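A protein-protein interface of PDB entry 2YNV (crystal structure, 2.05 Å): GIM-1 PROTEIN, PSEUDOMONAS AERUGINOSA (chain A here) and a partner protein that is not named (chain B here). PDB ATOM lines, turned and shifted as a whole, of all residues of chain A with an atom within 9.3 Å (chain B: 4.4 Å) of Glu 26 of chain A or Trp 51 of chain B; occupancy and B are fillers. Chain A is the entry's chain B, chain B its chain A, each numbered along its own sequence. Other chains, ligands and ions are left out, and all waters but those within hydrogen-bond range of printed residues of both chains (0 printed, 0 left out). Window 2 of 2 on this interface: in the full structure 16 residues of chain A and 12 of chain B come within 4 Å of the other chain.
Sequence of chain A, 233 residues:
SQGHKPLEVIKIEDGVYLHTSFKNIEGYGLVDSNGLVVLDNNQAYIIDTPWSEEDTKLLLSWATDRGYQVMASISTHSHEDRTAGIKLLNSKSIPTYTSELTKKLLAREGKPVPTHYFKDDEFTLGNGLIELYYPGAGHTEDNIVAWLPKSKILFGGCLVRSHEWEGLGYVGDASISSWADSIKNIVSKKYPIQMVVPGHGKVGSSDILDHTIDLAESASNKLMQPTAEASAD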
ATOM      1  N   LYS A  23      -1.450  26.772  -2.452  1.00  0.00           N
ATOM      2  CA  LYS A  23      -0.937  25.768  -3.363  1.00  0.00           C
ATOM      3  C   LYS A  23      -0.901  26.500  -4.692  1.00  0.00           C
ATOM      4  O   LYS A  23      -1.655  27.450  -4.952  1.00  0.00           O
ATOM      5  CB  LYS A  23      -1.831  24.514  -3.429  1.00  0.00           C
ATOM      6  CG  LYS A  23      -1.526  23.534  -4.576  1.00  0.00           C
ATOM      7  CD  LYS A  23      -0.220  22.763  -4.378  1.00  0.00           C
ATOM      8  CE  LYS A  23       0.059  21.826  -5.575  1.00  0.00           C
ATOM      9  NZ  LYS A  23       1.375  21.115  -5.517  1.00  0.00           N
ATOM     10  N   ASN A  24       0.012  26.085  -5.533  1.00  0.00           N
ATOM     11  CA  ASN A  24       0.369  26.940  -6.610  1.00  0.00           C
ATOM     12  C   ASN A  24       0.728  26.167  -7.831  1.00  0.00           C
ATOM     13  O   ASN A  24       0.577  24.935  -7.893  1.00  0.00           O
ATOM     14  CB  ASN A  24       1.545  27.796  -6.121  1.00  0.00           C
ATOM     15  CG  ASN A  24       2.275  27.162  -4.906  1.00  0.00           C
ATOM     16  OD1 ASN A  24       1.784  27.287  -3.789  1.00  0.00           O
ATOM     17  ND2 ASN A  24       3.427  26.521  -5.112  1.00  0.00           N
ATOM     18  N   ILE A  25       1.137  26.916  -8.837  1.00  0.00           N
ATOM     19  CA  ILE A  25       2.324  26.482  -9.543  1.00  0.00           C
ATOM     20  C   ILE A  25       2.329  25.760 -10.871  1.00  0.00           C
ATOM     21  O   ILE A  25       1.314  25.752 -11.573  1.00  0.00           O
ATOM     22  CB  ILE A  25       3.540  26.351  -8.557  1.00  0.00           C
ATOM     23  CG1 ILE A  25       4.714  27.257  -8.967  1.00  0.00           C
ATOM     24  CG2 ILE A  25       3.835  24.875  -8.175  1.00  0.00           C
ATOM     25  CD1 ILE A  25       5.335  27.977  -7.715  1.00  0.00           C
ATOM     26  N   GLU A  26       3.457  25.147 -11.207  1.00  0.00           N
ATOM     27  CA  GLU A  26       3.632  24.581 -12.544  1.00  0.00           C
ATOM     28  C   GLU A  26       2.932  25.455 -13.558  1.00  0.00           C
ATOM     29  O   GLU A  26       2.007  24.993 -14.205  1.00  0.00           O
ATOM     30  CB  GLU A  26       2.987  23.207 -12.658  1.00  0.00           C
ATOM     31  CG  GLU A  26       3.469  22.175 -11.689  1.00  0.00           C
ATOM     32  CD  GLU A  26       2.708  20.877 -11.864  1.00  0.00           C
ATOM     33  OE1 GLU A  26       2.994  20.152 -12.849  1.00  0.00           O
ATOM     34  OE2 GLU A  26       1.808  20.604 -11.030  1.00  0.00           O
ATOM     35  N   GLY A  27       3.331  26.712 -13.687  1.00  0.00           N
ATOM     36  CA  GLY A  27       2.816  27.531 -14.770  1.00  0.00           C
ATOM     37  C   GLY A  27       1.346  27.894 -14.666  1.00  0.00           C
ATOM     38  O   GLY A  27       0.689  28.209 -15.650  1.00  0.00           O
ATOM     39  N   TYR A  28       0.814  27.807 -13.465  1.00  0.00           N
ATOM     40  CA  TYR A  28      -0.334  28.604 -13.120  1.00  0.00           C
ATOM     41  C   TYR A  28       0.065  29.387 -11.882  1.00  0.00           C
ATOM     42  O   TYR A  28       1.009  29.002 -11.206  1.00  0.00           O
ATOM     43  CB  TYR A  28      -1.550  27.740 -12.831  1.00  0.00           C
ATOM     44  CG  TYR A  28      -2.762  28.609 -12.673  1.00  0.00           C
ATOM     45  CD1 TYR A  28      -3.281  29.287 -13.776  1.00  0.00           C
ATOM     46  CD2 TYR A  28      -3.354  28.810 -11.426  1.00  0.00           C
ATOM     47  CE1 TYR A  28      -4.366  30.116 -13.651  1.00  0.00           C
ATOM     48  CE2 TYR A  28      -4.445  29.636 -11.290  1.00  0.00           C
ATOM     49  CZ  TYR A  28      -4.948  30.294 -12.403  1.00  0.00           C
ATOM     50  OH  TYR A  28      -6.042  31.125 -12.270  1.00  0.00           O
ATOM     51  N   GLY A  29      -0.656  30.467 -11.580  1.00  0.00           N
ATOM     52  CA  GLY A  29      -0.341  31.323 -10.436  1.00  0.00           C
ATOM     53  C   GLY A  29      -0.455  30.656  -9.069  1.00  0.00           C
ATOM     54  O   GLY A  29      -0.208  29.444  -8.920  1.00  0.00           O
ATOM     55  N   LEU A  30      -0.800  31.461  -8.061  1.00  0.00           N
ATOM     56  CA  LEU A  30      -1.022  30.946  -6.694  1.00  0.00           C
ATOM     57  C   LEU A  30      -2.501  30.793  -6.368  1.00  0.00           C
ATOM     58  O   LEU A  30      -3.266  31.765  -6.422  1.00  0.00           O
ATOM     59  CB  LEU A  30      -0.412  31.855  -5.622  1.00  0.00           C
ATOM     60  CG  LEU A  30       1.097  32.074  -5.538  1.00  0.00           C
ATOM     61  CD1 LEU A  30       1.421  32.958  -4.338  1.00  0.00           C
ATOM     62  CD2 LEU A  30       1.855  30.777  -5.453  1.00  0.00           C
ATOM     63  N   SER B  21      -2.468  20.621 -23.533  1.00  0.00           N
ATOM     64  CA  SER B  21      -2.828  19.713 -22.470  1.00  0.00           C
ATOM     65  C   SER B  21      -3.503  20.501 -21.360  1.00  0.00           C
ATOM     66  O   SER B  21      -3.336  21.732 -21.243  1.00  0.00           O
ATOM     67  CB  SER B  21      -1.638  18.900 -21.966  1.00  0.00           C
ATOM     68  OG  SER B  21      -0.418  19.607 -21.895  1.00  0.00           O
ATOM     69  N   LYS B  23      -4.891  20.803 -17.217  1.00  0.00           N
ATOM     70  CA  LYS B  23      -4.989  20.421 -15.810  1.00  0.00           C
ATOM     71  C   LYS B  23      -6.153  21.169 -15.148  1.00  0.00           C
ATOM     72  O   LYS B  23      -6.388  22.346 -15.403  1.00  0.00           O
ATOM     73  CB  LYS B  23      -3.680  20.668 -15.053  1.00  0.00           C
ATOM     74  CG  LYS B  23      -3.742  20.229 -13.601  1.00  0.00           C
ATOM     75  N   VAL B  31      -7.200  24.763 -16.780  1.00  0.00           N
ATOM     76  CA  VAL B  31      -6.087  25.536 -17.264  1.00  0.00           C
ATOM     77  C   VAL B  31      -5.453  24.706 -18.393  1.00  0.00           C
ATOM     78  O   VAL B  31      -5.354  23.470 -18.310  1.00  0.00           O
ATOM     79  CB  VAL B  31      -5.153  25.805 -16.082  1.00  0.00           C
ATOM     80  CG1 VAL B  31      -5.981  26.286 -14.934  1.00  0.00           C
ATOM     81  CG2 VAL B  31      -4.432  24.541 -15.616  1.00  0.00           C
ATOM     82  N   ASP B  32      -5.087  25.367 -19.476  1.00  0.00           N
ATOM     83  CA  ASP B  32      -4.473  24.681 -20.594  1.00  0.00           C
ATOM     84  C   ASP B  32      -2.984  25.066 -20.585  1.00  0.00           C
ATOM     85  O   ASP B  32      -2.590  25.996 -19.853  1.00  0.00           O
ATOM     86  CB  ASP B  32      -5.123  25.194 -21.834  1.00  0.00           C
ATOM     87  CG  ASP B  32      -4.721  26.617 -22.102  1.00  0.00           C
ATOM     88  OD1 ASP B  32      -3.541  26.920 -21.821  1.00  0.00           O
ATOM     89  OD2 ASP B  32      -5.542  27.424 -22.546  1.00  0.00           O
ATOM     90  N   SER B  33      -2.183  24.366 -21.391  1.00  0.00           N
ATOM     91  CA  SER B  33      -0.780  24.649 -21.614  1.00  0.00           C
ATOM     92  C   SER B  33      -0.428  24.242 -23.046  1.00  0.00           C
ATOM     93  O   SER B  33      -0.807  23.148 -23.491  1.00  0.00           O
ATOM     94  CB  SER B  33       0.050  23.797 -20.687  1.00  0.00           C
ATOM     95  OG  SER B  33       1.418  24.044 -20.921  1.00  0.00           O
ATOM     96  N   THR B  49       7.031  19.834 -23.892  1.00  0.00           N
ATOM     97  CA  THR B  49       6.389  18.562 -23.676  1.00  0.00           C
ATOM     98  C   THR B  49       5.076  18.945 -23.059  1.00  0.00           C
ATOM     99  O   THR B  49       4.891  20.095 -22.639  1.00  0.00           O
ATOM    100  CB  THR B  49       7.230  17.623 -22.733  1.00  0.00           C
ATOM    101  OG1 THR B  49       7.242  18.117 -21.388  1.00  0.00           O
ATOM    102  CG2 THR B  49       8.671  17.520 -23.224  1.00  0.00           C
ATOM    103  N   PRO B  50       4.104  18.060 -23.137  1.00  0.00           N
ATOM    104  CA  PRO B  50       2.849  18.309 -22.439  1.00  0.00           C
ATOM    105  C   PRO B  50       3.104  18.324 -20.963  1.00  0.00           C
ATOM    106  O   PRO B  50       4.205  17.998 -20.562  1.00  0.00           O
ATOM    107  CB  PRO B  50       2.001  17.073 -22.785  1.00  0.00           C
ATOM    108  CG  PRO B  50       2.528  16.630 -24.064  1.00  0.00           C
ATOM    109  CD  PRO B  50       3.986  16.952 -24.080  1.00  0.00           C
ATOM    110  N   TRP B  51       2.059  18.628 -20.206  1.00  0.00           N
ATOM    111  CA  TRP B  51       2.127  18.965 -18.808  1.00  0.00           C
ATOM    112  C   TRP B  51       2.248  17.714 -17.926  1.00  0.00           C
ATOM    113  O   TRP B  51       2.388  17.812 -16.718  1.00  0.00           O
ATOM    114  CB  TRP B  51       0.845  19.715 -18.491  1.00  0.00           C
ATOM    115  CG  TRP B  51       0.916  20.660 -17.380  1.00  0.00           C
ATOM    116  CD1 TRP B  51       1.815  20.669 -16.335  1.00  0.00           C
ATOM    117  CD2 TRP B  51       0.030  21.764 -17.160  1.00  0.00           C
ATOM    118  NE1 TRP B  51       1.526  21.713 -15.477  1.00  0.00           N
ATOM    119  CE2 TRP B  51       0.439  22.400 -15.959  1.00  0.00           C
ATOM    120  CE3 TRP B  51      -1.072  22.275 -17.857  1.00  0.00           C
ATOM    121  CZ2 TRP B  51      -0.209  23.535 -15.460  1.00  0.00           C
ATOM    122  CZ3 TRP B  51      -1.720  23.392 -17.359  1.00  0.00           C
ATOM    123  CH2 TRP B  51      -1.287  24.015 -16.172  1.00  0.00           C
ATOM    124  N   SER B  52       2.187  16.534 -18.534  1.00  0.00           N
ATOM    125  CA  SER B  52       2.223  15.300 -17.757  1.00  0.00           C
ATOM    126  C   SER B  52       2.858  14.179 -18.590  1.00  0.00           C
ATOM    127  O   SER B  52       2.854  14.275 -19.817  1.00  0.00           O
ATOM    128  CB  SER B  52       0.795  14.913 -17.362  1.00  0.00           C
ATOM    129  OG  SER B  52       0.104  14.353 -18.468  1.00  0.00           O
ATOM    130  N   GLU B  80       7.556  22.526 -14.856  1.00  0.00           N
ATOM    131  CA  GLU B  80       6.834  21.339 -15.246  1.00  0.00           C
ATOM    132  C   GLU B  80       5.997  21.367 -16.512  1.00  0.00           C
ATOM    133  O   GLU B  80       6.004  20.363 -17.270  1.00  0.00           O
ATOM    134  CB  GLU B  80       5.951  20.888 -14.115  1.00  0.00           C
ATOM    135  CG  GLU B  80       6.138  19.464 -13.942  1.00  0.00           C
ATOM    136  CD  GLU B  80       7.561  19.169 -13.569  1.00  0.00           C
ATOM    137  OE1 GLU B  80       8.218  20.094 -13.039  1.00  0.00           O
ATOM    138  OE2 GLU B  80       8.019  18.031 -13.800  1.00  0.00           O
ATOM    139  N   ASP B  81       5.282  22.472 -16.755  1.00  0.00           N
ATOM    140  CA  ASP B  81       4.465  22.575 -17.983  1.00  0.00           C
ATOM    141  C   ASP B  81       5.314  22.560 -19.267  1.00  0.00           C
ATOM    142  O   ASP B  81       4.770  22.598 -20.384  1.00  0.00           O
ATOM    143  CB  ASP B  81       3.528  23.810 -17.998  1.00  0.00           C
ATOM    144  CG  ASP B  81       4.255  25.131 -17.768  1.00  0.00           C
ATOM    145  OD1 ASP B  81       5.231  25.162 -16.996  1.00  0.00           O
ATOM    146  OD2 ASP B  81       3.808  26.154 -18.344  1.00  0.00           O
ATOM    147  N   ALA B  84       7.779  18.064 -18.281  1.00  0.00           N
ATOM    148  CA  ALA B  84       7.232  16.867 -17.656  1.00  0.00           C
ATOM    149  C   ALA B  84       7.585  15.601 -18.449  1.00  0.00           C
ATOM    150  O   ALA B  84       7.878  14.537 -17.890  1.00  0.00           O
ATOM    151  CB  ALA B  84       5.739  17.026 -17.543  1.00  0.00           C
ATOM    152  N   HIS B 200       0.263  29.537 -22.526  1.00  0.00           N
ATOM    153  CA  HIS B 200      -1.108  29.314 -22.021  1.00  0.00           C
ATOM    154  C   HIS B 200      -2.035  30.300 -22.665  1.00  0.00           C
ATOM    155  O   HIS B 200      -1.738  31.493 -22.721  1.00  0.00           O
ATOM    156  CB  HIS B 200      -1.227  29.470 -20.494  1.00  0.00           C
ATOM    157  CG  HIS B 200      -0.250  28.649 -19.712  1.00  0.00           C
ATOM    158  ND1 HIS B 200      -0.513  27.365 -19.288  1.00  0.00           N
ATOM    159  CD2 HIS B 200       0.977  28.952 -19.228  1.00  0.00           C
ATOM    160  CE1 HIS B 200       0.542  26.886 -18.643  1.00  0.00           C
ATOM    161  NE2 HIS B 200       1.450  27.842 -18.570  1.00  0.00           N
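Of the 13 printed residues of chain B, 4 touch a printed residue of chain A.
Among the printed residues, no Asp or Glu carboxylate lies within 4 Å of a Lys or Arg side-chain nitrogen of the other chain.
OG of Ser 21 of chain B is in hydrogen-bond range of N of Trp 51 of chain B, 3.2 Å away.
A ring nitrogen (ND1) of His 200 of chain B is in hydrogen-bond range of the backbone carbonyl oxygen (O) of Asp 32 of chain B (2.6 Å).
OD2 of Asp 81 of chain B sits at hydrogen-bond distance from NE2 of His 200 of chain B (2.9 Å).
The side-chain carboxylate of Glu 26 of chain A sits at hydrogen-bond distance from the indole nitrogen of Trp 51 of chain B, 3.4 Å away.
NE2 of His 200 of chain B is in hydrogen-bond range of O of Gly 27 of chain A (3.0 Å).
Among the printed residues, pairs that only touch across the chains: Glu 26 of chain A with Glu 80 of chain B (3.3 Å) and Gly 27 of chain A with Asp 81 of chain B (3.96 Å).
Glu 26 of chain A touches just these residues of chain B: Trp 51 and Glu 80.
Of chain A, only Glu 26 (2.9 Å) comes within 4 Å of Trp 51 of chain B.
No residue of chain A comes within 4 Å of Ser 52 of chain B.
Asp 81 of chain B touches one residue of chain A.
Of the printed residues of chain A, Glu 80 of chain B touches Glu 26 (3.3 Å).
Of the printed residues of chain A, His 200 of chain B touches Gly 27 (3.0 Å).
Of the printed residues of chain B, Gly 27 of chain A touches Asp 81 (3.96 Å) and His 200 (3.0 Å).
Asn 24 of chain A touches none of the printed residues of chain B.
Val 31 of chain B touches none of the printed residues of chain A.
The nearest residue of chain B that does not touch Glu 26 of chain A is Asp 81 of chain B (4.1 Å).
The nearest residue of chain A that does not touch Trp 51 of chain B is Gly 27 of chain A (4.7 Å).
The nearest printed residue of chain B that does not touch Gly 27 of chain A is Trp 51 of chain B (4.7 Å).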
